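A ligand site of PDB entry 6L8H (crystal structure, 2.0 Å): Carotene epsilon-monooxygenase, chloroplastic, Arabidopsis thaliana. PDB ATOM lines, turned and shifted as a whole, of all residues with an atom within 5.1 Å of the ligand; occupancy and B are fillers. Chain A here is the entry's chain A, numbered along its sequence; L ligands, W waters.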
ATOM      1  N   LEU A  66      23.712 -20.889  -3.411  1.00  0.00           N
ATOM      2  CA  LEU A  66      22.900 -19.685  -3.313  1.00  0.00           C
ATOM      3  C   LEU A  66      23.668 -18.451  -3.777  1.00  0.00           C
ATOM      4  O   LEU A  66      23.110 -17.564  -4.426  1.00  0.00           O
ATOM      5  CB  LEU A  66      22.410 -19.510  -1.863  1.00  0.00           C
ATOM      6  CG  LEU A  66      21.363 -20.578  -1.490  1.00  0.00           C
ATOM      7  CD1 LEU A  66      21.039 -20.584  -0.017  1.00  0.00           C
ATOM      8  CD2 LEU A  66      20.073 -20.411  -2.286  1.00  0.00           C
ATOM      9  N   LYS A  74      16.608 -20.266 -10.961  1.00  0.00           N
ATOM     10  CA  LYS A  74      15.458 -20.540 -10.100  1.00  0.00           C
ATOM     11  C   LYS A  74      14.829 -21.890 -10.397  1.00  0.00           C
ATOM     12  O   LYS A  74      14.164 -22.437  -9.507  1.00  0.00           O
ATOM     13  CB  LYS A  74      14.403 -19.447 -10.222  1.00  0.00           C
ATOM     14  CG  LYS A  74      14.874 -18.117  -9.628  1.00  0.00           C
ATOM     15  CD  LYS A  74      14.652 -18.077  -8.140  1.00  0.00           C
ATOM     16  CE  LYS A  74      13.150 -18.100  -7.832  1.00  0.00           C
ATOM     17  NZ  LYS A  74      12.925 -17.949  -6.372  1.00  0.00           N
ATOM     18  N   PHE A  89       8.867 -10.124 -10.446  1.00  0.00           N
ATOM     19  CA  PHE A  89      10.310 -10.343 -10.353  1.00  0.00           C
ATOM     20  C   PHE A  89      10.695 -11.397  -9.318  1.00  0.00           C
ATOM     21  O   PHE A  89      11.853 -11.817  -9.322  1.00  0.00           O
ATOM     22  CB  PHE A  89      11.059  -9.036 -10.050  1.00  0.00           C
ATOM     23  CG  PHE A  89      11.014  -8.571  -8.606  1.00  0.00           C
ATOM     24  CD1 PHE A  89       9.879  -7.946  -8.092  1.00  0.00           C
ATOM     25  CD2 PHE A  89      12.126  -8.712  -7.795  1.00  0.00           C
ATOM     26  CE1 PHE A  89       9.845  -7.497  -6.764  1.00  0.00           C
ATOM     27  CE2 PHE A  89      12.113  -8.259  -6.470  1.00  0.00           C
ATOM     28  CZ  PHE A  89      10.975  -7.647  -5.959  1.00  0.00           C
ATOM     29  N   ALA A  90       9.781 -11.852  -8.451  1.00  0.00           N
ATOM     30  CA  ALA A  90      10.165 -12.945  -7.551  1.00  0.00           C
ATOM     31  C   ALA A  90      10.453 -14.241  -8.305  1.00  0.00           C
ATOM     32  O   ALA A  90      11.172 -15.094  -7.778  1.00  0.00           O
ATOM     33  CB  ALA A  90       9.088 -13.200  -6.494  1.00  0.00           C
ATOM     34  N   TRP A  97      14.560  -9.350 -14.407  1.00  0.00           N
ATOM     35  CA  TRP A  97      14.755  -9.500 -12.967  1.00  0.00           C
ATOM     36  C   TRP A  97      15.733  -8.463 -12.424  1.00  0.00           C
ATOM     37  O   TRP A  97      15.416  -7.748 -11.461  1.00  0.00           O
ATOM     38  CB  TRP A  97      15.219 -10.911 -12.638  1.00  0.00           C
ATOM     39  CG  TRP A  97      15.672 -11.020 -11.237  1.00  0.00           C
ATOM     40  CD1 TRP A  97      14.900 -11.078 -10.106  1.00  0.00           C
ATOM     41  CD2 TRP A  97      17.035 -11.015 -10.781  1.00  0.00           C
ATOM     42  NE1 TRP A  97      15.686 -11.134  -8.986  1.00  0.00           N
ATOM     43  CE2 TRP A  97      17.005 -11.088  -9.382  1.00  0.00           C
ATOM     44  CE3 TRP A  97      18.275 -10.964 -11.438  1.00  0.00           C
ATOM     45  CZ2 TRP A  97      18.177 -11.127  -8.606  1.00  0.00           C
ATOM     46  CZ3 TRP A  97      19.427 -11.003 -10.676  1.00  0.00           C
ATOM     47  CH2 TRP A  97      19.367 -11.080  -9.269  1.00  0.00           C
ATOM     48  N   ARG A 101      14.202  -5.834  -9.663  1.00  0.00           N
ATOM     49  CA  ARG A 101      14.680  -5.876  -8.280  1.00  0.00           C
ATOM     50  C   ARG A 101      15.397  -4.573  -7.915  1.00  0.00           C
ATOM     51  O   ARG A 101      15.191  -4.020  -6.827  1.00  0.00           O
ATOM     52  CB  ARG A 101      15.568  -7.089  -8.046  1.00  0.00           C
ATOM     53  CG  ARG A 101      15.998  -7.269  -6.586  1.00  0.00           C
ATOM     54  CD  ARG A 101      16.857  -8.487  -6.397  1.00  0.00           C
ATOM     55  NE  ARG A 101      17.506  -8.499  -5.100  1.00  0.00           N
ATOM     56  CZ  ARG A 101      17.299  -9.394  -4.130  1.00  0.00           C
ATOM     57  NH1 ARG A 101      16.430 -10.407  -4.288  1.00  0.00           N
ATOM     58  NH2 ARG A 101      17.977  -9.279  -2.996  1.00  0.00           N
ATOM     59  N   LEU A 108      12.043  -0.009   0.037  1.00  0.00           N
ATOM     60  CA  LEU A 108      12.028  -0.575   1.388  1.00  0.00           C
ATOM     61  C   LEU A 108      12.992   0.132   2.333  1.00  0.00           C
ATOM     62  O   LEU A 108      13.644  -0.518   3.148  1.00  0.00           O
ATOM     63  CB  LEU A 108      12.323  -2.069   1.313  1.00  0.00           C
ATOM     64  CG  LEU A 108      11.251  -2.843   0.558  1.00  0.00           C
ATOM     65  CD1 LEU A 108      11.703  -4.234   0.068  1.00  0.00           C
ATOM     66  CD2 LEU A 108      10.014  -2.975   1.411  1.00  0.00           C
ATOM     67  N   ILE A 156       0.436  -6.813   4.866  1.00  0.00           N
ATOM     68  CA  ILE A 156       1.134  -6.691   3.596  1.00  0.00           C
ATOM     69  C   ILE A 156       0.320  -5.846   2.611  1.00  0.00           C
ATOM     70  O   ILE A 156       0.868  -5.037   1.870  1.00  0.00           O
ATOM     71  CB  ILE A 156       1.525  -8.067   3.027  1.00  0.00           C
ATOM     72  CG1 ILE A 156       2.587  -7.902   1.929  1.00  0.00           C
ATOM     73  CG2 ILE A 156       0.295  -8.855   2.511  1.00  0.00           C
ATOM     74  CD1 ILE A 156       3.926  -7.453   2.455  1.00  0.00           C
ATOM     75  N   ILE A 253       4.347   1.065  -0.904  1.00  0.00           N
ATOM     76  CA  ILE A 253       5.340   0.761  -1.919  1.00  0.00           C
ATOM     77  C   ILE A 253       4.812   1.102  -3.311  1.00  0.00           C
ATOM     78  O   ILE A 253       5.562   1.602  -4.158  1.00  0.00           O
ATOM     79  CB  ILE A 253       5.780  -0.718  -1.799  1.00  0.00           C
ATOM     80  CG1 ILE A 253       6.685  -0.868  -0.560  1.00  0.00           C
ATOM     81  CG2 ILE A 253       6.487  -1.223  -3.083  1.00  0.00           C
ATOM     82  CD1 ILE A 253       6.801  -2.277  -0.070  1.00  0.00           C
ATOM     83  N   SER A 275       3.676 -10.620  -6.571  1.00  0.00           N
ATOM     84  CA  SER A 275       4.678 -11.510  -6.023  1.00  0.00           C
ATOM     85  C   SER A 275       5.095 -11.092  -4.610  1.00  0.00           C
ATOM     86  O   SER A 275       5.363 -11.959  -3.767  1.00  0.00           O
ATOM     87  CB  SER A 275       5.873 -11.619  -6.979  1.00  0.00           C
ATOM     88  OG  SER A 275       6.749 -10.501  -6.944  1.00  0.00           O
ATOM     89  N   MET A 276       5.118  -9.787  -4.322  1.00  0.00           N
ATOM     90  CA  MET A 276       5.443  -9.339  -2.964  1.00  0.00           C
ATOM     91  C   MET A 276       4.308  -9.619  -2.001  1.00  0.00           C
ATOM     92  O   MET A 276       4.565  -9.906  -0.821  1.00  0.00           O
ATOM     93  CB  MET A 276       5.799  -7.859  -2.938  1.00  0.00           C
ATOM     94  CG  MET A 276       6.985  -7.559  -3.838  1.00  0.00           C
ATOM     95  SD  MET A 276       7.339  -5.829  -4.009  1.00  0.00           S
ATOM     96  CE  MET A 276       7.955  -5.447  -2.350  1.00  0.00           C
ATOM     97  N   ALA A 279       4.812 -13.211  -1.238  1.00  0.00           N
ATOM     98  CA  ALA A 279       6.061 -13.461  -0.525  1.00  0.00           C
ATOM     99  C   ALA A 279       5.995 -12.978   0.922  1.00  0.00           C
ATOM    100  O   ALA A 279       6.597 -13.608   1.810  1.00  0.00           O
ATOM    101  CB  ALA A 279       7.231 -12.789  -1.246  1.00  0.00           C
ATOM    102  N   GLY A 280       5.246 -11.912   1.200  1.00  0.00           N
ATOM    103  CA  GLY A 280       5.211 -11.280   2.507  1.00  0.00           C
ATOM    104  C   GLY A 280       4.101 -11.699   3.474  1.00  0.00           C
ATOM    105  O   GLY A 280       4.120 -11.295   4.622  1.00  0.00           O
ATOM    106  N   THR A 283       4.479 -16.535   4.962  1.00  0.00           N
ATOM    107  CA  THR A 283       5.750 -16.669   5.669  1.00  0.00           C
ATOM    108  C   THR A 283       5.721 -15.968   7.023  1.00  0.00           C
ATOM    109  O   THR A 283       6.033 -16.562   8.068  1.00  0.00           O
ATOM    110  CB  THR A 283       6.884 -16.081   4.835  1.00  0.00           C
ATOM    111  OG1 THR A 283       6.484 -14.804   4.324  1.00  0.00           O
ATOM    112  CG2 THR A 283       7.313 -17.027   3.694  1.00  0.00           C
ATOM    113  N   THR A 284       5.419 -14.674   7.013  1.00  0.00           N
ATOM    114  CA  THR A 284       5.396 -13.918   8.261  1.00  0.00           C
ATOM    115  C   THR A 284       4.373 -14.501   9.237  1.00  0.00           C
ATOM    116  O   THR A 284       4.625 -14.550  10.445  1.00  0.00           O
ATOM    117  CB  THR A 284       5.092 -12.442   7.979  1.00  0.00           C
ATOM    118  OG1 THR A 284       5.856 -11.999   6.852  1.00  0.00           O
ATOM    119  CG2 THR A 284       5.454 -11.559   9.202  1.00  0.00           C
ATOM    120  N   VAL A 287       5.929 -17.681  10.768  1.00  0.00           N
ATOM    121  CA  VAL A 287       6.956 -17.344  11.759  1.00  0.00           C
ATOM    122  C   VAL A 287       6.297 -16.976  13.086  1.00  0.00           C
ATOM    123  O   VAL A 287       6.731 -17.433  14.157  1.00  0.00           O
ATOM    124  CB  VAL A 287       7.848 -16.190  11.268  1.00  0.00           C
ATOM    125  CG1 VAL A 287       8.736 -15.675  12.434  1.00  0.00           C
ATOM    126  CG2 VAL A 287       8.733 -16.611  10.061  1.00  0.00           C
ATOM    127  N   MET A 337      12.661 -19.316  13.541  1.00  0.00           N
ATOM    128  CA  MET A 337      12.948 -19.532  12.124  1.00  0.00           C
ATOM    129  C   MET A 337      14.016 -20.607  11.906  1.00  0.00           C
ATOM    130  O   MET A 337      13.997 -21.286  10.876  1.00  0.00           O
ATOM    131  CB  MET A 337      13.357 -18.217  11.458  1.00  0.00           C
ATOM    132  CG  MET A 337      12.257 -17.136  11.586  1.00  0.00           C
ATOM    133  SD  MET A 337      12.498 -15.623  10.608  1.00  0.00           S
ATOM    134  CE  MET A 337      12.520 -16.345   8.938  1.00  0.00           C
ATOM    135  N   HIS A 342      10.714 -21.269   6.530  1.00  0.00           N
ATOM    136  CA  HIS A 342       9.665 -21.128   5.534  1.00  0.00           C
ATOM    137  C   HIS A 342      10.238 -20.560   4.248  1.00  0.00           C
ATOM    138  O   HIS A 342      10.788 -19.437   4.269  1.00  0.00           O
ATOM    139  CB  HIS A 342       8.557 -20.224   6.070  1.00  0.00           C
ATOM    140  CG  HIS A 342       8.180 -20.513   7.500  1.00  0.00           C
ATOM    141  ND1 HIS A 342       7.428 -21.611   7.856  1.00  0.00           N
ATOM    142  CD2 HIS A 342       8.433 -19.843   8.644  1.00  0.00           C
ATOM    143  CE1 HIS A 342       7.250 -21.607   9.165  1.00  0.00           C
ATOM    144  NE2 HIS A 342       7.825 -20.529   9.666  1.00  0.00           N
ATOM    145  N   PRO A 343      10.215 -21.286   3.116  1.00  0.00           N
ATOM    146  CA  PRO A 343       9.847 -22.692   3.012  1.00  0.00           C
ATOM    147  C   PRO A 343      10.980 -23.578   3.543  1.00  0.00           C
ATOM    148  O   PRO A 343      12.101 -23.126   3.736  1.00  0.00           O
ATOM    149  CB  PRO A 343       9.667 -22.874   1.504  1.00  0.00           C
ATOM    150  CG  PRO A 343      10.644 -21.919   0.925  1.00  0.00           C
ATOM    151  CD  PRO A 343      10.808 -20.789   1.862  1.00  0.00           C
ATOM    152  N   LEU A 346      14.732 -24.900  -0.471  1.00  0.00           N
ATOM    153  CA  LEU A 346      14.965 -23.927  -1.533  1.00  0.00           C
ATOM    154  C   LEU A 346      15.340 -24.685  -2.799  1.00  0.00           C
ATOM    155  O   LEU A 346      16.032 -25.711  -2.733  1.00  0.00           O
ATOM    156  CB  LEU A 346      16.108 -22.956  -1.159  1.00  0.00           C
ATOM    157  CG  LEU A 346      15.923 -22.147   0.131  1.00  0.00           C
ATOM    158  CD1 LEU A 346      17.187 -21.323   0.455  1.00  0.00           C
ATOM    159  CD2 LEU A 346      14.684 -21.240  -0.041  1.00  0.00           C
ATOM    160  N   ILE A 347      14.859 -24.208  -3.946  1.00  0.00           N
ATOM    161  CA  ILE A 347      14.996 -24.909  -5.219  1.00  0.00           C
ATOM    162  C   ILE A 347      15.916 -24.102  -6.138  1.00  0.00           C
ATOM    163  O   ILE A 347      15.835 -22.878  -6.188  1.00  0.00           O
ATOM    164  CB  ILE A 347      13.629 -25.147  -5.888  1.00  0.00           C
ATOM    165  CG1 ILE A 347      12.703 -25.919  -4.961  1.00  0.00           C
ATOM    166  CG2 ILE A 347      13.798 -25.877  -7.243  1.00  0.00           C
ATOM    167  CD1 ILE A 347      13.192 -27.307  -4.648  1.00  0.00           C
ATOM    168  N   ARG A 348      16.803 -24.814  -6.844  1.00  0.00           N
ATOM    169  CA  ARG A 348      17.646 -24.207  -7.883  1.00  0.00           C
ATOM    170  C   ARG A 348      17.767 -25.205  -9.026  1.00  0.00           C
ATOM    171  O   ARG A 348      17.258 -26.335  -8.962  1.00  0.00           O
ATOM    172  CB  ARG A 348      19.039 -23.807  -7.346  1.00  0.00           C
ATOM    173  CG  ARG A 348      19.049 -22.601  -6.373  1.00  0.00           C
ATOM    174  CD  ARG A 348      18.509 -21.335  -7.071  1.00  0.00           C
ATOM    175  NE  ARG A 348      18.705 -20.127  -6.255  1.00  0.00           N
ATOM    176  CZ  ARG A 348      17.802 -19.635  -5.402  1.00  0.00           C
ATOM    177  NH1 ARG A 348      16.623 -20.230  -5.229  1.00  0.00           N
ATOM    178  NH2 ARG A 348      18.098 -18.523  -4.708  1.00  0.00           N
ATOM    179  N   PRO A 411      17.621 -17.969   7.302  1.00  0.00           N
ATOM    180  CA  PRO A 411      16.206 -17.627   7.462  1.00  0.00           C
ATOM    181  C   PRO A 411      15.580 -16.946   6.250  1.00  0.00           C
ATOM    182  O   PRO A 411      14.363 -17.046   6.069  1.00  0.00           O
ATOM    183  CB  PRO A 411      16.213 -16.684   8.680  1.00  0.00           C
ATOM    184  CG  PRO A 411      17.563 -16.070   8.670  1.00  0.00           C
ATOM    185  CD  PRO A 411      18.507 -17.127   8.118  1.00  0.00           C
ATOM    186  N   PHE A 412      16.370 -16.295   5.390  1.00  0.00           N
ATOM    187  CA  PHE A 412      15.848 -15.440   4.325  1.00  0.00           C
ATOM    188  C   PHE A 412      16.566 -15.726   3.017  1.00  0.00           C
ATOM    189  O   PHE A 412      16.774 -14.815   2.183  1.00  0.00           O
ATOM    190  CB  PHE A 412      15.977 -13.962   4.707  1.00  0.00           C
ATOM    191  CG  PHE A 412      15.048 -13.535   5.804  1.00  0.00           C
ATOM    192  CD1 PHE A 412      13.668 -13.502   5.588  1.00  0.00           C
ATOM    193  CD2 PHE A 412      15.534 -13.165   7.044  1.00  0.00           C
ATOM    194  CE1 PHE A 412      12.799 -13.113   6.592  1.00  0.00           C
ATOM    195  CE2 PHE A 412      14.650 -12.752   8.082  1.00  0.00           C
ATOM    196  CZ  PHE A 412      13.279 -12.729   7.841  1.00  0.00           C
ATOM    197  N   SER A 413      16.959 -16.981   2.812  1.00  0.00           N
ATOM    198  CA  SER A 413      17.789 -17.414   1.687  1.00  0.00           C
ATOM    199  C   SER A 413      19.096 -16.621   1.644  1.00  0.00           C
ATOM    200  O   SER A 413      19.540 -16.118   2.680  1.00  0.00           O
ATOM    201  CB  SER A 413      17.008 -17.305   0.383  1.00  0.00           C
ATOM    202  OG  SER A 413      17.679 -17.939  -0.691  1.00  0.00           O
ATOM    203  N   PRO A 416      22.289 -13.540  -4.623  1.00  0.00           N
ATOM    204  CA  PRO A 416      21.586 -12.486  -5.393  1.00  0.00           C
ATOM    205  C   PRO A 416      20.070 -12.541  -5.296  1.00  0.00           C
ATOM    206  O   PRO A 416      19.448 -11.489  -5.421  1.00  0.00           O
ATOM    207  CB  PRO A 416      22.071 -12.715  -6.832  1.00  0.00           C
ATOM    208  CG  PRO A 416      23.512 -13.298  -6.642  1.00  0.00           C
ATOM    209  CD  PRO A 416      23.402 -14.158  -5.382  1.00  0.00           C
ATOM    210  N   ARG A 417      19.465 -13.725  -5.044  1.00  0.00           N
ATOM    211  CA  ARG A 417      18.035 -13.872  -4.903  1.00  0.00           C
ATOM    212  C   ARG A 417      17.556 -13.817  -3.452  1.00  0.00           C
ATOM    213  O   ARG A 417      16.431 -14.226  -3.176  1.00  0.00           O
ATOM    214  CB  ARG A 417      17.545 -15.198  -5.528  1.00  0.00           C
ATOM    215  CG  ARG A 417      17.892 -15.464  -7.018  1.00  0.00           C
ATOM    216  CD  ARG A 417      17.354 -14.397  -7.979  1.00  0.00           C
ATOM    217  NE  ARG A 417      15.882 -14.339  -8.060  1.00  0.00           N
ATOM    218  CZ  ARG A 417      15.175 -14.310  -9.186  1.00  0.00           C
ATOM    219  NH1 ARG A 417      15.783 -14.411 -10.369  1.00  0.00           N
ATOM    220  NH2 ARG A 417      13.835 -14.253  -9.148  1.00  0.00           N
ATOM    221  N   LYS A 418      18.391 -13.358  -2.525  1.00  0.00           N
ATOM    222  CA  LYS A 418      17.975 -13.219  -1.125  1.00  0.00           C
ATOM    223  C   LYS A 418      16.656 -12.462  -1.006  1.00  0.00           C
ATOM    224  O   LYS A 418      16.379 -11.535  -1.788  1.00  0.00           O
ATOM    225  CB  LYS A 418      19.066 -12.493  -0.338  1.00  0.00           C
ATOM    226  CG  LYS A 418      18.866 -12.519   1.164  1.00  0.00           C
ATOM    227  CD  LYS A 418      19.959 -11.763   1.917  1.00  0.00           C
ATOM    228  CE  LYS A 418      19.623 -11.732   3.428  1.00  0.00           C
ATOM    229  NZ  LYS A 418      20.740 -11.113   4.239  1.00  0.00           N
ATOM    230  N   CYS A 419      15.826 -12.864  -0.023  1.00  0.00           N
ATOM    231  CA  CYS A 419      14.581 -12.155   0.293  1.00  0.00           C
ATOM    232  C   CYS A 419      14.825 -10.647   0.423  1.00  0.00           C
ATOM    233  O   CYS A 419      15.721 -10.219   1.145  1.00  0.00           O
ATOM    234  CB  CYS A 419      13.997 -12.682   1.600  1.00  0.00           C
ATOM    235  SG  CYS A 419      12.584 -11.697   2.250  1.00  0.00           S
ATOM    236  N   VAL A 420      14.003  -9.852  -0.270  1.00  0.00           N
ATOM    237  CA  VAL A 420      14.109  -8.399  -0.153  1.00  0.00           C
ATOM    238  C   VAL A 420      13.307  -7.826   1.014  1.00  0.00           C
ATOM    239  O   VAL A 420      13.539  -6.673   1.415  1.00  0.00           O
ATOM    240  CB  VAL A 420      13.689  -7.656  -1.451  1.00  0.00           C
ATOM    241  CG1 VAL A 420      14.545  -8.072  -2.630  1.00  0.00           C
ATOM    242  CG2 VAL A 420      12.221  -7.858  -1.732  1.00  0.00           C
ATOM    243  N   GLY A 421      12.405  -8.610   1.600  1.00  0.00           N
ATOM    244  CA  GLY A 421      11.633  -8.154   2.742  1.00  0.00           C
ATOM    245  C   GLY A 421      12.156  -8.631   4.090  1.00  0.00           C
ATOM    246  O   GLY A 421      11.388  -8.662   5.054  1.00  0.00           O
ATOM    247  N   PHE A 424      11.968  -5.857   6.684  1.00  0.00           N
ATOM    248  CA  PHE A 424      10.541  -5.609   6.843  1.00  0.00           C
ATOM    249  C   PHE A 424       9.880  -6.685   7.689  1.00  0.00           C
ATOM    250  O   PHE A 424       9.175  -6.402   8.657  1.00  0.00           O
ATOM    251  CB  PHE A 424       9.885  -5.537   5.458  1.00  0.00           C
ATOM    252  CG  PHE A 424       8.413  -5.254   5.449  1.00  0.00           C
ATOM    253  CD1 PHE A 424       7.491  -6.204   5.832  1.00  0.00           C
ATOM    254  CD2 PHE A 424       7.951  -4.035   4.973  1.00  0.00           C
ATOM    255  CE1 PHE A 424       6.111  -5.939   5.803  1.00  0.00           C
ATOM    256  CE2 PHE A 424       6.588  -3.756   4.913  1.00  0.00           C
ATOM    257  CZ  PHE A 424       5.656  -4.702   5.338  1.00  0.00           C
ATOM    258  N   ALA A 425      10.079  -7.950   7.303  1.00  0.00           N
ATOM    259  CA  ALA A 425       9.363  -9.031   7.946  1.00  0.00           C
ATOM    260  C   ALA A 425       9.805  -9.215   9.388  1.00  0.00           C
ATOM    261  O   ALA A 425       8.970  -9.487  10.264  1.00  0.00           O
ATOM    262  CB  ALA A 425       9.576 -10.337   7.165  1.00  0.00           C
HETATM  263  C1  LIG L   1      12.356 -14.157  -1.591  1.00  0.00           C
HETATM  264  C2  LIG L   1      11.451 -15.852   2.863  1.00  0.00           C
HETATM  265  C3  LIG L   1       8.972 -11.837   4.091  1.00  0.00           C
HETATM  266  C4  LIG L   1       9.465 -10.368  -0.512  1.00  0.00           C
HETATM  267  C5  LIG L   1      12.374 -14.934  -0.448  1.00  0.00           C
HETATM  268  C6  LIG L   1      13.140 -16.144  -0.259  1.00  0.00           C
HETATM  269  C7  LIG L   1      12.907 -16.612   0.966  1.00  0.00           C
HETATM  270  C8  LIG L   1      11.965 -15.709   1.600  1.00  0.00           C
HETATM  271  C9  LIG L   1      13.523 -17.879   1.618  1.00  0.00           C
HETATM  272  C10 LIG L   1      14.106 -16.686  -1.334  1.00  0.00           C
HETATM  273  C11 LIG L   1      13.542 -17.821  -2.140  1.00  0.00           C
HETATM  274  C12 LIG L   1      14.674 -18.272  -3.042  1.00  0.00           C
HETATM  275  O1  LIG L   1      15.859 -17.786  -2.937  1.00  0.00           O
HETATM  276  O2  LIG L   1      14.347 -19.106  -3.903  1.00  0.00           O
HETATM  277  C13 LIG L   1      10.723 -14.913   3.595  1.00  0.00           C
HETATM  278  C14 LIG L   1      10.282 -15.061   4.977  1.00  0.00           C
HETATM  279  C15 LIG L   1       9.579 -13.980   5.310  1.00  0.00           C
HETATM  280  C16 LIG L   1       9.573 -13.087   4.167  1.00  0.00           C
HETATM  281  C17 LIG L   1      10.594 -16.313   5.820  1.00  0.00           C
HETATM  282  C18 LIG L   1       8.908 -13.608   6.655  1.00  0.00           C
HETATM  283  C19 LIG L   1       9.358 -14.049   7.826  1.00  0.00           C
HETATM  284  C20 LIG L   1       8.903 -11.065   2.943  1.00  0.00           C
HETATM  285  C21 LIG L   1       8.240  -9.794   2.826  1.00  0.00           C
HETATM  286  C22 LIG L   1       8.358  -9.382   1.547  1.00  0.00           C
HETATM  287  C23 LIG L   1       9.107 -10.387   0.830  1.00  0.00           C
HETATM  288  C24 LIG L   1       7.534  -9.117   4.015  1.00  0.00           C
HETATM  289  C25 LIG L   1       7.866  -8.074   0.886  1.00  0.00           C
HETATM  290  C26 LIG L   1       7.703  -6.931   1.579  1.00  0.00           C
HETATM  291  C27 LIG L   1      10.252 -11.274  -1.207  1.00  0.00           C
HETATM  292  C28 LIG L   1      10.554 -11.213  -2.621  1.00  0.00           C
HETATM  293  C29 LIG L   1      11.372 -12.247  -2.922  1.00  0.00           C
HETATM  294  C30 LIG L   1      11.585 -13.007  -1.711  1.00  0.00           C
HETATM  295  C31 LIG L   1      10.037 -10.118  -3.586  1.00  0.00           C
HETATM  296  C32 LIG L   1      11.976 -12.608  -4.299  1.00  0.00           C
HETATM  297  C33 LIG L   1      13.390 -12.017  -4.376  1.00  0.00           C
HETATM  298  C34 LIG L   1      14.062 -12.313  -5.702  1.00  0.00           C
HETATM  299  O3  LIG L   1      14.810 -11.429  -6.175  1.00  0.00           O
HETATM  300  O4  LIG L   1      13.862 -13.421  -6.298  1.00  0.00           O
HETATM  301  N1  LIG L   1      11.650 -14.701   0.697  1.00  0.00           N
HETATM  302  N2  LIG L   1      10.254 -13.707   3.145  1.00  0.00           N
HETATM  303  N3  LIG L   1       9.406 -11.401   1.707  1.00  0.00           N
HETATM  304  N4  LIG L   1      10.902 -12.379  -0.693  1.00  0.00           N
HETATM  305 FE1  LIG L   1      10.738 -12.940   1.256  1.00  0.00          FE
HETATM  306  O   HOH W   1      14.086 -15.659  -4.634  1.00  0.00           O
HETATM  307  O   HOH W   2      13.241 -21.970  -3.928  1.00  0.00           O
HETATM  308  O   HOH W   3       8.859 -14.630   0.669  1.00  0.00           O
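The side-chain sulfur (SG) of Cys 419 is bound to an iron atom (FE1) of the ligand (2.4 Å). An oxygen (O3) of the ligand lies within salt-bridge range of the guanidinium group of Arg 101 (2.7 Å). An oxygen (O4) of the ligand lies within salt-bridge range of the guanidinium group (NE) of Arg 417 (2.8 Å). O2 of the ligand is in salt-bridge range of NH1 of Arg 348 (2.9 Å). OG of Ser 413 sits at hydrogen-bond distance from O1 of the ligand (2.9 Å). NE1 of Trp 97 sits at hydrogen-bond distance from O3 of the ligand, at 3.0 Å. O2 of the ligand lies within salt-bridge range of NZ of Lys 74, 3.1 Å away.
Water W1 lies within hydrogen-bond range of O4 of the ligand, NZ of Lys 74 and O of Arg 417. Water W2 lies within hydrogen-bond range of N of Ile 347 (2.8 Å) and O2 of the ligand (3.1 Å).
The backbone carbonyl oxygen (O) of Ala 90 lies close to an oxygen (O4) of the ligand (3.5 Å). Phe 89 touches the ligand. Ile 156 touches the ligand. CG of Met 276 touches C31 of the ligand, 3.99 Å away. CB of Ala 279 touches C4 of the ligand, at 3.4 Å. CA of Gly 280 touches C21 of the ligand, 3.4 Å away. OG1 of Thr 283 touches C15 of the ligand, at 3.4 Å. Thr 284 touches the ligand. Val 287 touches the ligand (CG2 to C19, 3.5 Å). CE of Met 337 touches C17 of the ligand (3.7 Å). His 342 touches the ligand (O to C17, 3.5 Å). Pro 343 touches the ligand (CD to C9, 3.99 Å). CD2 of Leu 346 touches C9 of the ligand, 3.9 Å away. O of Pro 411 touches C17 of the ligand, at 3.8 Å. CE1 of Phe 412 touches C14 of the ligand (3.6 Å). Lys 418 touches the ligand (O to C33, 3.98 Å). Val 420 touches the ligand (CG2 to C31, 3.6 Å). CA of Gly 421 touches C22 of the ligand, 3.7 Å away. Phe 424 touches the ligand. CB of Ala 425 touches C18 of the ligand, at 3.4 Å. Hydrophobic or aromatic side chains within 4 Å of the ligand: Phe 89, Ala 90, Trp 97, Ile 156, Met 276, Ala 279, Val 287, Met 337, Pro 343, Leu 346, Phe 412, Val 420, Phe 424 and Ala 425. The nearest printed residue that does not touch the ligand is Leu 108 (4.6 Å).
The backbone NH (N) of Cys 419 sits at hydrogen-bond distance from the backbone carbonyl oxygen (O) of Phe 412 (3.1 Å). The side-chain sulfur (SG) of Cys 419 sits close to the backbone NH (N) of Gly 421, at 3.2 Å. The guanidinium group (NH1) of Arg 101 lies within hydrogen-bond range of the backbone carbonyl oxygen (O) of Lys 418, at 2.7 Å. NH1 of Arg 101 lies close to O of Pro 416 (3.4 Å). O of Ala 90 sits at hydrogen-bond distance from NH2 of Arg 417 (3.1 Å). NH2 of Arg 417 lies within hydrogen-bond range of O of Phe 89 (3.1 Å). The backbone carbonyl oxygen of Ala 279 is in hydrogen-bond range of the side-chain hydroxyl of Thr 283, at 2.8 Å. The side-chain hydroxyl of Thr 284 is in hydrogen-bond range of the backbone carbonyl oxygen of Gly 280, at 2.9 Å.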
